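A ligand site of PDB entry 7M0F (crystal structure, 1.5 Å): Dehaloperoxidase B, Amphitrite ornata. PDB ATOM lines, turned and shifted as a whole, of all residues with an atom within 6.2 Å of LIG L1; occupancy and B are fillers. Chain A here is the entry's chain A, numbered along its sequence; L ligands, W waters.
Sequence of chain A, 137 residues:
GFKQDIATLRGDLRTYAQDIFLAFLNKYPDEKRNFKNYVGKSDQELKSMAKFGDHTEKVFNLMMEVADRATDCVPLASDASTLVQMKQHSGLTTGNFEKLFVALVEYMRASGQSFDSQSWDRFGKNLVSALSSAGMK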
ATOM      1  N   PHE A  21     -22.799  -9.201 -22.308  1.00  0.00           N
ATOM      2  CA  PHE A  21     -24.128  -9.103 -21.711  1.00  0.00           C
ATOM      3  C   PHE A  21     -25.218  -9.316 -22.768  1.00  0.00           C
ATOM      4  O   PHE A  21     -26.230  -9.970 -22.496  1.00  0.00           O
ATOM      5  CB  PHE A  21     -24.310  -7.771 -20.992  1.00  0.00           C
ATOM      6  CG  PHE A  21     -25.623  -7.641 -20.265  1.00  0.00           C
ATOM      7  CD1 PHE A  21     -26.027  -8.607 -19.364  1.00  0.00           C
ATOM      8  CD2 PHE A  21     -26.438  -6.541 -20.477  1.00  0.00           C
ATOM      9  CE1 PHE A  21     -27.227  -8.494 -18.690  1.00  0.00           C
ATOM     10  CE2 PHE A  21     -27.648  -6.406 -19.811  1.00  0.00           C
ATOM     11  CZ  PHE A  21     -28.044  -7.393 -18.912  1.00  0.00           C
ATOM     12  N   PHE A  24     -25.573 -12.931 -23.409  1.00  0.00           N
ATOM     13  CA  PHE A  24     -26.352 -13.511 -22.324  1.00  0.00           C
ATOM     14  C   PHE A  24     -27.853 -13.281 -22.516  1.00  0.00           C
ATOM     15  O   PHE A  24     -28.649 -14.240 -22.487  1.00  0.00           O
ATOM     16  CB  PHE A  24     -25.865 -12.906 -20.998  1.00  0.00           C
ATOM     17  CG  PHE A  24     -26.783 -13.124 -19.826  1.00  0.00           C
ATOM     18  CD1 PHE A  24     -26.919 -14.371 -19.229  1.00  0.00           C
ATOM     19  CD2 PHE A  24     -27.457 -12.050 -19.272  1.00  0.00           C
ATOM     20  CE1 PHE A  24     -27.743 -14.535 -18.115  1.00  0.00           C
ATOM     21  CE2 PHE A  24     -28.283 -12.214 -18.168  1.00  0.00           C
ATOM     22  CZ  PHE A  24     -28.413 -13.467 -17.582  1.00  0.00           C
ATOM     23  N   GLU A  31     -34.258 -14.275 -19.116  1.00  0.00           N
ATOM     24  CA  GLU A  31     -33.529 -13.505 -18.108  1.00  0.00           C
ATOM     25  C   GLU A  31     -33.905 -12.024 -18.101  1.00  0.00           C
ATOM     26  O   GLU A  31     -33.587 -11.321 -17.147  1.00  0.00           O
ATOM     27  CB  GLU A  31     -32.026 -13.718 -18.242  1.00  0.00           C
ATOM     28  CG  GLU A  31     -31.584 -15.152 -17.894  1.00  0.00           C
ATOM     29  CD  GLU A  31     -31.645 -15.440 -16.401  1.00  0.00           C
ATOM     30  OE1 GLU A  31     -32.274 -16.440 -15.998  1.00  0.00           O
ATOM     31  OE2 GLU A  31     -31.049 -14.666 -15.632  1.00  0.00           O
ATOM     32  N   ASN A  34     -35.530  -9.890 -15.115  1.00  0.00           N
ATOM     33  CA  ASN A  34     -34.817  -9.011 -14.213  1.00  0.00           C
ATOM     34  C   ASN A  34     -34.341  -7.718 -14.865  1.00  0.00           C
ATOM     35  O   ASN A  34     -33.670  -6.918 -14.191  1.00  0.00           O
ATOM     36  CB  ASN A  34     -33.599  -9.736 -13.601  1.00  0.00           C
ATOM     37  CG  ASN A  34     -33.992 -10.743 -12.540  1.00  0.00           C
ATOM     38  OD1 ASN A  34     -34.701 -10.424 -11.600  1.00  0.00           O
ATOM     39  ND2 ASN A  34     -33.519 -11.969 -12.703  1.00  0.00           N
ATOM     40  N   PHE A  35     -34.675  -7.484 -16.139  1.00  0.00           N
ATOM     41  CA  PHE A  35     -34.228  -6.302 -16.890  1.00  0.00           C
ATOM     42  C   PHE A  35     -35.387  -5.731 -17.711  1.00  0.00           C
ATOM     43  O   PHE A  35     -35.360  -5.672 -18.938  1.00  0.00           O
ATOM     44  CB  PHE A  35     -33.019  -6.621 -17.775  1.00  0.00           C
ATOM     45  CG  PHE A  35     -31.857  -7.189 -17.016  1.00  0.00           C
ATOM     46  CD1 PHE A  35     -31.600  -8.548 -17.017  1.00  0.00           C
ATOM     47  CD2 PHE A  35     -31.017  -6.358 -16.282  1.00  0.00           C
ATOM     48  CE1 PHE A  35     -30.520  -9.075 -16.302  1.00  0.00           C
ATOM     49  CE2 PHE A  35     -29.947  -6.878 -15.575  1.00  0.00           C
ATOM     50  CZ  PHE A  35     -29.693  -8.236 -15.596  1.00  0.00           C
ATOM     51  N   TYR A  38     -34.831  -3.361 -20.656  1.00  0.00           N
ATOM     52  CA  TYR A  38     -34.122  -3.814 -21.844  1.00  0.00           C
ATOM     53  C   TYR A  38     -34.997  -4.618 -22.794  1.00  0.00           C
ATOM     54  O   TYR A  38     -34.519  -5.082 -23.835  1.00  0.00           O
ATOM     55  CB  TYR A  38     -32.863  -4.609 -21.445  1.00  0.00           C
ATOM     56  CG  TYR A  38     -31.872  -3.855 -20.580  1.00  0.00           C
ATOM     57  CD1 TYR A  38     -31.833  -2.453 -20.563  1.00  0.00           C
ATOM     58  CD2 TYR A  38     -30.960  -4.531 -19.785  1.00  0.00           C
ATOM     59  CE1 TYR A  38     -30.923  -1.771 -19.755  1.00  0.00           C
ATOM     60  CE2 TYR A  38     -30.051  -3.849 -18.987  1.00  0.00           C
ATOM     61  CZ  TYR A  38     -30.034  -2.482 -18.977  1.00  0.00           C
ATOM     62  OH  TYR A  38     -29.118  -1.821 -18.181  1.00  0.00           O
ATOM     63  N   LYS A  51     -28.187   3.966 -19.526  1.00  0.00           N
ATOM     64  CA  LYS A  51     -27.995   3.060 -18.403  1.00  0.00           C
ATOM     65  C   LYS A  51     -27.485   1.702 -18.851  1.00  0.00           C
ATOM     66  O   LYS A  51     -26.755   1.050 -18.102  1.00  0.00           O
ATOM     67  CB  LYS A  51     -29.280   2.920 -17.586  1.00  0.00           C
ATOM     68  CG  LYS A  51     -29.662   4.180 -16.829  1.00  0.00           C
ATOM     69  CD  LYS A  51     -30.889   3.949 -15.986  1.00  0.00           C
ATOM     70  CE  LYS A  51     -31.172   5.152 -15.106  1.00  0.00           C
ATOM     71  NZ  LYS A  51     -32.405   4.921 -14.292  1.00  0.00           N
ATOM     72  N   ASP A  54     -23.701   2.316 -19.255  1.00  0.00           N
ATOM     73  CA  ASP A  54     -23.033   2.673 -18.010  1.00  0.00           C
ATOM     74  C   ASP A  54     -23.107   1.544 -16.995  1.00  0.00           C
ATOM     75  O   ASP A  54     -22.099   1.222 -16.352  1.00  0.00           O
ATOM     76  CB  ASP A  54     -23.651   3.969 -17.462  1.00  0.00           C
ATOM     77  CG  ASP A  54     -23.254   5.201 -18.273  1.00  0.00           C
ATOM     78  OD1 ASP A  54     -22.258   5.169 -19.017  1.00  0.00           O
ATOM     79  OD2 ASP A  54     -23.954   6.232 -18.163  1.00  0.00           O
ATOM     80  N   HIS A  55     -24.275   0.917 -16.854  1.00  0.00           N
ATOM     81  CA  HIS A  55     -24.422  -0.150 -15.873  1.00  0.00           C
ATOM     82  C   HIS A  55     -23.644  -1.395 -16.289  1.00  0.00           C
ATOM     83  O   HIS A  55     -22.964  -2.002 -15.458  1.00  0.00           O
ATOM     84  CB  HIS A  55     -25.888  -0.485 -15.617  1.00  0.00           C
ATOM     85  CG  HIS A  55     -26.626   0.582 -14.877  1.00  0.00           C
ATOM     86  ND1 HIS A  55     -27.508   0.305 -13.857  1.00  0.00           N
ATOM     87  CD2 HIS A  55     -26.623   1.924 -15.019  1.00  0.00           C
ATOM     88  CE1 HIS A  55     -28.013   1.430 -13.395  1.00  0.00           C
ATOM     89  NE2 HIS A  55     -27.498   2.436 -14.082  1.00  0.00           N
ATOM     90  N   THR A  56     -23.705  -1.755 -17.570  1.00  0.00           N
ATOM     91  CA  THR A  56     -22.978  -2.930 -18.015  1.00  0.00           C
ATOM     92  C   THR A  56     -21.478  -2.758 -17.792  1.00  0.00           C
ATOM     93  O   THR A  56     -20.792  -3.691 -17.357  1.00  0.00           O
ATOM     94  CB  THR A  56     -23.312  -3.257 -19.466  1.00  0.00           C
ATOM     95  OG1 THR A  56     -24.736  -3.352 -19.620  1.00  0.00           O
ATOM     96  CG2 THR A  56     -22.662  -4.563 -19.889  1.00  0.00           C
ATOM     97  N   LYS A  58     -20.062  -0.803 -15.472  1.00  0.00           N
ATOM     98  CA  LYS A  58     -19.803  -0.888 -14.037  1.00  0.00           C
ATOM     99  C   LYS A  58     -19.863  -2.328 -13.530  1.00  0.00           C
ATOM    100  O   LYS A  58     -19.043  -2.718 -12.680  1.00  0.00           O
ATOM    101  CB  LYS A  58     -20.763   0.030 -13.278  1.00  0.00           C
ATOM    102  CG  LYS A  58     -20.288   1.466 -13.274  1.00  0.00           C
ATOM    103  CD  LYS A  58     -21.380   2.374 -12.755  1.00  0.00           C
ATOM    104  CE  LYS A  58     -20.914   3.821 -12.647  1.00  0.00           C
ATOM    105  NZ  LYS A  58     -22.043   4.739 -12.283  1.00  0.00           N
ATOM    106  N   VAL A  59     -20.780  -3.139 -14.065  1.00  0.00           N
ATOM    107  CA  VAL A  59     -20.820  -4.566 -13.715  1.00  0.00           C
ATOM    108  C   VAL A  59     -19.494  -5.224 -14.060  1.00  0.00           C
ATOM    109  O   VAL A  59     -18.905  -5.939 -13.233  1.00  0.00           O
ATOM    110  CB  VAL A  59     -21.981  -5.266 -14.444  1.00  0.00           C
ATOM    111  CG1 VAL A  59     -21.842  -6.800 -14.345  1.00  0.00           C
ATOM    112  CG2 VAL A  59     -23.343  -4.806 -13.913  1.00  0.00           C
ATOM    113  N   PHE A  60     -19.002  -4.975 -15.270  1.00  0.00           N
ATOM    114  CA  PHE A  60     -17.787  -5.640 -15.705  1.00  0.00           C
ATOM    115  C   PHE A  60     -16.534  -5.027 -15.078  1.00  0.00           C
ATOM    116  O   PHE A  60     -15.550  -5.739 -14.889  1.00  0.00           O
ATOM    117  CB  PHE A  60     -17.711  -5.726 -17.230  1.00  0.00           C
ATOM    118  CG  PHE A  60     -18.498  -6.880 -17.788  1.00  0.00           C
ATOM    119  CD1 PHE A  60     -17.858  -8.021 -18.266  1.00  0.00           C
ATOM    120  CD2 PHE A  60     -19.889  -6.858 -17.783  1.00  0.00           C
ATOM    121  CE1 PHE A  60     -18.607  -9.090 -18.758  1.00  0.00           C
ATOM    122  CE2 PHE A  60     -20.637  -7.927 -18.275  1.00  0.00           C
ATOM    123  CZ  PHE A  60     -19.991  -9.047 -18.753  1.00  0.00           C
ATOM    124  N   LEU A  62     -16.364  -4.182 -11.952  1.00  0.00           N
ATOM    125  CA  LEU A  62     -16.270  -4.910 -10.704  1.00  0.00           C
ATOM    126  C   LEU A  62     -15.954  -6.373 -10.944  1.00  0.00           C
ATOM    127  O   LEU A  62     -15.158  -6.965 -10.216  1.00  0.00           O
ATOM    128  CB  LEU A  62     -17.559  -4.747  -9.889  1.00  0.00           C
ATOM    129  CG  LEU A  62     -17.562  -5.348  -8.487  1.00  0.00           C
ATOM    130  CD1 LEU A  62     -16.403  -4.786  -7.679  1.00  0.00           C
ATOM    131  CD2 LEU A  62     -18.891  -5.047  -7.814  1.00  0.00           C
ATOM    132  N   MET A  63     -16.551  -6.968 -11.983  1.00  0.00           N
ATOM    133  CA  MET A  63     -16.256  -8.366 -12.278  1.00  0.00           C
ATOM    134  C   MET A  63     -14.762  -8.569 -12.492  1.00  0.00           C
ATOM    135  O   MET A  63     -14.191  -9.551 -11.995  1.00  0.00           O
ATOM    136  CB  MET A  63     -17.040  -8.869 -13.483  1.00  0.00           C
ATOM    137  CG  MET A  63     -16.921 -10.381 -13.706  1.00  0.00           C
ATOM    138  SD  MET A  63     -17.320 -10.930 -15.385  1.00  0.00           S
ATOM    139  CE  MET A  63     -19.068 -10.556 -15.413  1.00  0.00           C
ATOM    140  N   MET A  64     -14.101  -7.644 -13.189  1.00  0.00           N
ATOM    141  CA  MET A  64     -12.669  -7.798 -13.450  1.00  0.00           C
ATOM    142  C   MET A  64     -11.864  -7.657 -12.166  1.00  0.00           C
ATOM    143  O   MET A  64     -10.829  -8.325 -12.007  1.00  0.00           O
ATOM    144  CB  MET A  64     -12.192  -6.817 -14.528  1.00  0.00           C
ATOM    145  CG  MET A  64     -12.745  -7.060 -15.945  1.00  0.00           C
ATOM    146  SD  MET A  64     -12.438  -8.724 -16.564  1.00  0.00           S
ATOM    147  CE  MET A  64     -14.008  -9.538 -16.228  1.00  0.00           C
ATOM    148  N   VAL A  66     -12.985  -8.553  -9.148  1.00  0.00           N
ATOM    149  CA  VAL A  66     -13.197  -9.825  -8.465  1.00  0.00           C
ATOM    150  C   VAL A  66     -12.316 -10.906  -9.070  1.00  0.00           C
ATOM    151  O   VAL A  66     -11.655 -11.665  -8.361  1.00  0.00           O
ATOM    152  CB  VAL A  66     -14.687 -10.195  -8.490  1.00  0.00           C
ATOM    153  CG1 VAL A  66     -14.913 -11.584  -7.940  1.00  0.00           C
ATOM    154  CG2 VAL A  66     -15.508  -9.190  -7.665  1.00  0.00           C
ATOM    155  N   LEU A  83     -21.362  -9.282  -3.371  1.00  0.00           N
ATOM    156  CA  LEU A  83     -22.279  -9.538  -4.473  1.00  0.00           C
ATOM    157  C   LEU A  83     -23.613 -10.081  -3.983  1.00  0.00           C
ATOM    158  O   LEU A  83     -24.656  -9.790  -4.588  1.00  0.00           O
ATOM    159  CB  LEU A  83     -21.650 -10.516  -5.465  1.00  0.00           C
ATOM    160  CG  LEU A  83     -20.466  -9.961  -6.242  1.00  0.00           C
ATOM    161  CD1 LEU A  83     -19.798 -11.101  -6.990  1.00  0.00           C
ATOM    162  CD2 LEU A  83     -20.913  -8.863  -7.198  1.00  0.00           C
ATOM    163  N   MET A  86     -25.528  -6.814  -2.024  1.00  0.00           N
ATOM    164  CA  MET A  86     -25.905  -5.628  -2.788  1.00  0.00           C
ATOM    165  C   MET A  86     -27.420  -5.555  -2.930  1.00  0.00           C
ATOM    166  O   MET A  86     -28.069  -6.556  -3.266  1.00  0.00           O
ATOM    167  CB  MET A  86     -25.272  -5.701  -4.186  1.00  0.00           C
ATOM    168  CG  MET A  86     -23.848  -5.153  -4.286  1.00  0.00           C
ATOM    169  SD  MET A  86     -23.082  -5.464  -5.900  1.00  0.00           S
ATOM    170  CE  MET A  86     -24.196  -4.580  -6.987  1.00  0.00           C
ATOM    171  N   GLN A  88     -29.135  -4.143  -5.243  1.00  0.00           N
ATOM    172  CA  GLN A  88     -29.508  -4.410  -6.624  1.00  0.00           C
ATOM    173  C   GLN A  88     -29.527  -5.894  -6.962  1.00  0.00           C
ATOM    174  O   GLN A  88     -29.990  -6.264  -8.042  1.00  0.00           O
ATOM    175  CB  GLN A  88     -28.571  -3.653  -7.562  1.00  0.00           C
ATOM    176  CG  GLN A  88     -28.826  -2.152  -7.598  1.00  0.00           C
ATOM    177  CD  GLN A  88     -27.653  -1.372  -8.133  1.00  0.00           C
ATOM    178  OE1 GLN A  88     -26.544  -1.447  -7.596  1.00  0.00           O
ATOM    179  NE2 GLN A  88     -27.872  -0.610  -9.203  1.00  0.00           N
ATOM    180  N   HIS A  89     -29.022  -6.754  -6.072  1.00  0.00           N
ATOM    181  CA  HIS A  89     -29.027  -8.192  -6.289  1.00  0.00           C
ATOM    182  C   HIS A  89     -30.070  -8.921  -5.442  1.00  0.00           C
ATOM    183  O   HIS A  89     -30.045 -10.153  -5.395  1.00  0.00           O
ATOM    184  CB  HIS A  89     -27.641  -8.767  -6.012  1.00  0.00           C
ATOM    185  CG  HIS A  89     -26.649  -8.465  -7.084  1.00  0.00           C
ATOM    186  ND1 HIS A  89     -25.311  -8.803  -6.975  1.00  0.00           N
ATOM    187  CD2 HIS A  89     -26.787  -7.867  -8.285  1.00  0.00           C
ATOM    188  CE1 HIS A  89     -24.678  -8.433  -8.067  1.00  0.00           C
ATOM    189  NE2 HIS A  89     -25.546  -7.854  -8.872  1.00  0.00           N
ATOM    190  N   LEU A  92     -31.965 -12.060  -6.954  1.00  0.00           N
ATOM    191  CA  LEU A  92     -31.193 -12.968  -7.788  1.00  0.00           C
ATOM    192  C   LEU A  92     -30.929 -14.290  -7.077  1.00  0.00           C
ATOM    193  O   LEU A  92     -30.919 -14.370  -5.848  1.00  0.00           O
ATOM    194  CB  LEU A  92     -29.862 -12.322  -8.163  1.00  0.00           C
ATOM    195  CG  LEU A  92     -30.013 -10.961  -8.845  1.00  0.00           C
ATOM    196  CD1 LEU A  92     -28.684 -10.448  -9.294  1.00  0.00           C
ATOM    197  CD2 LEU A  92     -30.964 -11.061 -10.018  1.00  0.00           C
ATOM    198  N   ASN A  96     -28.852 -17.270 -12.056  1.00  0.00           N
ATOM    199  CA  ASN A  96     -28.627 -16.085 -12.876  1.00  0.00           C
ATOM    200  C   ASN A  96     -27.140 -15.918 -13.202  1.00  0.00           C
ATOM    201  O   ASN A  96     -26.780 -15.618 -14.344  1.00  0.00           O
ATOM    202  CB  ASN A  96     -29.142 -14.820 -12.175  1.00  0.00           C
ATOM    203  CG  ASN A  96     -30.639 -14.851 -11.905  1.00  0.00           C
ATOM    204  OD1 ASN A  96     -31.068 -14.785 -10.761  1.00  0.00           O
ATOM    205  ND2 ASN A  96     -31.433 -14.942 -12.976  1.00  0.00           N
ATOM    206  N   PHE A  97     -26.285 -16.113 -12.211  1.00  0.00           N
ATOM    207  CA  PHE A  97     -24.837 -16.014 -12.418  1.00  0.00           C
ATOM    208  C   PHE A  97     -24.307 -17.176 -13.242  1.00  0.00           C
ATOM    209  O   PHE A  97     -23.425 -16.983 -14.091  1.00  0.00           O
ATOM    210  CB  PHE A  97     -24.130 -15.949 -11.056  1.00  0.00           C
ATOM    211  CG  PHE A  97     -24.371 -14.669 -10.316  1.00  0.00           C
ATOM    212  CD1 PHE A  97     -23.399 -13.671 -10.287  1.00  0.00           C
ATOM    213  CD2 PHE A  97     -25.578 -14.442  -9.658  1.00  0.00           C
ATOM    214  CE1 PHE A  97     -23.618 -12.488  -9.594  1.00  0.00           C
ATOM    215  CE2 PHE A  97     -25.798 -13.259  -8.975  1.00  0.00           C
ATOM    216  CZ  PHE A  97     -24.826 -12.275  -8.946  1.00  0.00           C
ATOM    217  N   GLU A  98     -24.808 -18.388 -13.001  1.00  0.00           N
ATOM    218  CA  GLU A  98     -24.400 -19.541 -13.791  1.00  0.00           C
ATOM    219  C   GLU A  98     -24.630 -19.284 -15.269  1.00  0.00           C
ATOM    220  O   GLU A  98     -23.753 -19.537 -16.107  1.00  0.00           O
ATOM    221  CB  GLU A  98     -25.183 -20.774 -13.333  1.00  0.00           C
ATOM    222  CG  GLU A  98     -24.613 -22.109 -13.802  1.00  0.00           C
ATOM    223  CD  GLU A  98     -25.089 -22.527 -15.187  1.00  0.00           C
ATOM    224  OE1 GLU A  98     -26.030 -21.895 -15.723  1.00  0.00           O
ATOM    225  OE2 GLU A  98     -24.534 -23.506 -15.736  1.00  0.00           O
ATOM    226  N   LEU A 100     -25.001 -16.325 -16.826  1.00  0.00           N
ATOM    227  CA  LEU A 100     -24.103 -15.299 -17.322  1.00  0.00           C
ATOM    228  C   LEU A 100     -22.761 -15.884 -17.719  1.00  0.00           C
ATOM    229  O   LEU A 100     -22.213 -15.553 -18.776  1.00  0.00           O
ATOM    230  CB  LEU A 100     -23.913 -14.193 -16.283  1.00  0.00           C
ATOM    231  CG  LEU A 100     -22.973 -13.035 -16.651  1.00  0.00           C
ATOM    232  CD1 LEU A 100     -23.488 -12.257 -17.867  1.00  0.00           C
ATOM    233  CD2 LEU A 100     -22.782 -12.096 -15.453  1.00  0.00           C
ATOM    234  N   PHE A 101     -22.214 -16.764 -16.879  1.00  0.00           N
ATOM    235  CA  PHE A 101     -20.873 -17.288 -17.162  1.00  0.00           C
ATOM    236  C   PHE A 101     -20.874 -18.309 -18.287  1.00  0.00           C
ATOM    237  O   PHE A 101     -19.892 -18.399 -19.040  1.00  0.00           O
ATOM    238  CB  PHE A 101     -20.141 -17.723 -15.878  1.00  0.00           C
ATOM    239  CG  PHE A 101     -19.594 -16.554 -15.141  1.00  0.00           C
ATOM    240  CD1 PHE A 101     -20.348 -15.876 -14.183  1.00  0.00           C
ATOM    241  CD2 PHE A 101     -18.341 -16.061 -15.464  1.00  0.00           C
ATOM    242  CE1 PHE A 101     -19.847 -14.762 -13.550  1.00  0.00           C
ATOM    243  CE2 PHE A 101     -17.840 -14.946 -14.831  1.00  0.00           C
ATOM    244  CZ  PHE A 101     -18.592 -14.297 -13.864  1.00  0.00           C
ATOM    245  N   PHE A 123     -13.883 -20.167 -13.107  1.00  0.00           N
ATOM    246  CA  PHE A 123     -14.179 -18.968 -12.328  1.00  0.00           C
ATOM    247  C   PHE A 123     -15.680 -18.799 -12.124  1.00  0.00           C
ATOM    248  O   PHE A 123     -16.140 -18.507 -11.019  1.00  0.00           O
ATOM    249  CB  PHE A 123     -13.570 -17.733 -13.017  1.00  0.00           C
ATOM    250  CG  PHE A 123     -13.888 -16.432 -12.333  1.00  0.00           C
ATOM    251  CD1 PHE A 123     -14.644 -15.452 -12.967  1.00  0.00           C
ATOM    252  CD2 PHE A 123     -13.426 -16.181 -11.051  1.00  0.00           C
ATOM    253  CE1 PHE A 123     -14.932 -14.241 -12.332  1.00  0.00           C
ATOM    254  CE2 PHE A 123     -13.718 -14.992 -10.405  1.00  0.00           C
ATOM    255  CZ  PHE A 123     -14.469 -14.018 -11.051  1.00  0.00           C
ATOM    256  N   LEU A 127     -17.321 -18.927  -8.558  1.00  0.00           N
ATOM    257  CA  LEU A 127     -18.079 -17.783  -8.057  1.00  0.00           C
ATOM    258  C   LEU A 127     -19.464 -18.228  -7.585  1.00  0.00           C
ATOM    259  O   LEU A 127     -19.915 -17.799  -6.519  1.00  0.00           O
ATOM    260  CB  LEU A 127     -18.182 -16.692  -9.131  1.00  0.00           C
ATOM    261  CG  LEU A 127     -19.012 -15.470  -8.726  1.00  0.00           C
ATOM    262  CD1 LEU A 127     -18.380 -14.736  -7.558  1.00  0.00           C
ATOM    263  CD2 LEU A 127     -19.190 -14.547  -9.923  1.00  0.00           C
HETATM  264  C1  LIG L   1     -26.379  -3.969 -10.634  1.00  0.00           C
HETATM  265  C2  LIG L   1     -21.997  -6.097 -10.355  1.00  0.00           C
HETATM  266  C3  LIG L   1     -23.969 -10.228 -11.926  1.00  0.00           C
HETATM  267  C4  LIG L   1     -28.379  -8.164 -11.988  1.00  0.00           C
HETATM  268  C5  LIG L   1     -25.012  -4.166 -10.497  1.00  0.00           C
HETATM  269  C6  LIG L   1     -24.019  -3.131 -10.277  1.00  0.00           C
HETATM  270  C7  LIG L   1     -22.816  -3.706 -10.199  1.00  0.00           C
HETATM  271  C8  LIG L   1     -23.000  -5.136 -10.371  1.00  0.00           C
HETATM  272  C9  LIG L   1     -21.472  -2.979  -9.973  1.00  0.00           C
HETATM  273  C10 LIG L   1     -24.318  -1.621 -10.162  1.00  0.00           C
HETATM  274  C11 LIG L   1     -24.531  -1.083 -11.575  1.00  0.00           C
HETATM  275  C12 LIG L   1     -24.887   0.379 -11.582  1.00  0.00           C
HETATM  276  O1  LIG L   1     -24.404   1.093 -12.494  1.00  0.00           O
HETATM  277  O2  LIG L   1     -25.650   0.810 -10.680  1.00  0.00           O
HETATM  278  C13 LIG L   1     -22.119  -7.404 -10.780  1.00  0.00           C
HETATM  279  C14 LIG L   1     -21.047  -8.373 -10.931  1.00  0.00           C
HETATM  280  C15 LIG L   1     -21.599  -9.522 -11.391  1.00  0.00           C
HETATM  281  C16 LIG L   1     -23.032  -9.314 -11.495  1.00  0.00           C
HETATM  282  C17 LIG L   1     -19.570  -8.047 -10.649  1.00  0.00           C
HETATM  283  C18 LIG L   1     -20.945 -10.886 -11.725  1.00  0.00           C
HETATM  284  C19 LIG L   1     -19.760 -11.275 -11.261  1.00  0.00           C
HETATM  285  C20 LIG L   1     -25.317 -10.007 -12.148  1.00  0.00           C
HETATM  286  C21 LIG L   1     -26.238 -10.958 -12.726  1.00  0.00           C
HETATM  287  C22 LIG L   1     -27.457 -10.385 -12.741  1.00  0.00           C
HETATM  288  C23 LIG L   1     -27.335  -9.069 -12.162  1.00  0.00           C
HETATM  289  C24 LIG L   1     -25.835 -12.361 -13.216  1.00  0.00           C
HETATM  290  C25 LIG L   1     -28.802 -10.940 -13.278  1.00  0.00           C
HETATM  291  C26 LIG L   1     -28.931 -11.930 -14.163  1.00  0.00           C
HETATM  292  C27 LIG L   1     -28.245  -6.847 -11.615  1.00  0.00           C
HETATM  293  C28 LIG L   1     -29.308  -5.870 -11.528  1.00  0.00           C
HETATM  294  C29 LIG L   1     -28.772  -4.690 -11.145  1.00  0.00           C
HETATM  295  C30 LIG L   1     -27.323  -4.906 -10.993  1.00  0.00           C
HETATM  296  C31 LIG L   1     -30.790  -6.189 -11.798  1.00  0.00           C
HETATM  297  C32 LIG L   1     -29.525  -3.347 -10.915  1.00  0.00           C
HETATM  298  C33 LIG L   1     -30.279  -2.858 -12.153  1.00  0.00           C
HETATM  299  C34 LIG L   1     -29.307  -2.527 -13.250  1.00  0.00           C
HETATM  300  O3  LIG L   1     -28.183  -2.072 -12.907  1.00  0.00           O
HETATM  301  O4  LIG L   1     -29.676  -2.700 -14.446  1.00  0.00           O
HETATM  302  N1  LIG L   1     -24.361  -5.376 -10.561  1.00  0.00           N
HETATM  303  N2  LIG L   1     -23.309  -8.017 -11.125  1.00  0.00           N
HETATM  304  N3  LIG L   1     -26.017  -8.856 -11.791  1.00  0.00           N
HETATM  305  N4  LIG L   1     -27.050  -6.227 -11.282  1.00  0.00           N
HETATM  306 FE1  LIG L   1     -25.234  -7.194 -10.975  1.00  0.00          FE
HETATM  307  O1  LG2 L   2     -27.527  -3.169 -16.016  1.00  0.00           O
HETATM  308  C1  LG2 L   2     -26.947  -4.442 -15.936  1.00  0.00           C
HETATM  309  C2  LG2 L   2     -26.182  -4.897 -16.982  1.00  0.00           C
HETATM  310  C3  LG2 L   2     -25.599  -6.149 -16.922  1.00  0.00           C
HETATM  311  C4  LG2 L   2     -25.792  -6.946 -15.793  1.00  0.00           C
HETATM  312  C5  LG2 L   2     -26.556  -6.477 -14.736  1.00  0.00           C
HETATM  313  C6  LG2 L   2     -27.120  -5.217 -14.810  1.00  0.00           C
HETATM  314 BR1  LG2 L   2     -24.996  -8.679 -15.724  1.00  0.00          BR
HETATM  315  O   HOH W   1     -32.050 -12.264 -15.074  1.00  0.00           O
HETATM  316  O   HOH W   2     -32.133  -2.863 -15.257  1.00  0.00           O
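An oxygen (O4) of LIG L1 sits at hydrogen-bond distance from an oxygen (O1) of LG2 L2, at 2.7 Å.
Residues that only touch LIG L1: Phe 97 (3.3 Å), Lys 58 (3.3 Å), Val 59 (3.4 Å), Leu 92 (3.5 Å), Met 63 (3.5 Å), Asn 96 (3.5 Å), Leu 127 (3.6 Å), Met 86 (3.6 Å), Phe 35 (3.7 Å), Glu 31 (3.8 Å), Leu 83 (3.8 Å), Phe 24 (3.8 Å), Leu 100 (3.8 Å), Asn 34 (3.8 Å), Tyr 38 (3.9 Å) and Leu 62 (3.9 Å).
Hydrophobic or aromatic side chains within 4 Å of LIG L1: Phe 24, Phe 35, His 55, Val 59, Leu 62, Met 63, Leu 83, Met 86, His 89, Leu 92, Phe 97, Leu 100 and Leu 127.
The backbone carbonyl oxygen of Leu 83 is in hydrogen-bond range of a ring nitrogen (ND1) of His 89.
The side-chain amide nitrogen (ND2) of Asn 96 lies within hydrogen-bond range of the side-chain carboxylate (OE2) of Glu 31.
Water W1 lies within hydrogen-bond range of the side-chain carboxylate of Glu 31, the side-chain amide nitrogen of Asn 34 and the side-chain amide nitrogen of Asn 96.
NE2 of His 89 binds FE1 of LIG L1, at 2.2 Å.
The side-chain hydroxyl (OH) of Tyr 38 lies within hydrogen-bond range of an oxygen (O1) of LG2 L2.
O3 of LIG L1 sits at hydrogen-bond distance from ND1 of His 55 (2.6 Å).
O2 of LIG L1 sits at hydrogen-bond distance from NE2 of Gln 88, 3.0 Å away.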
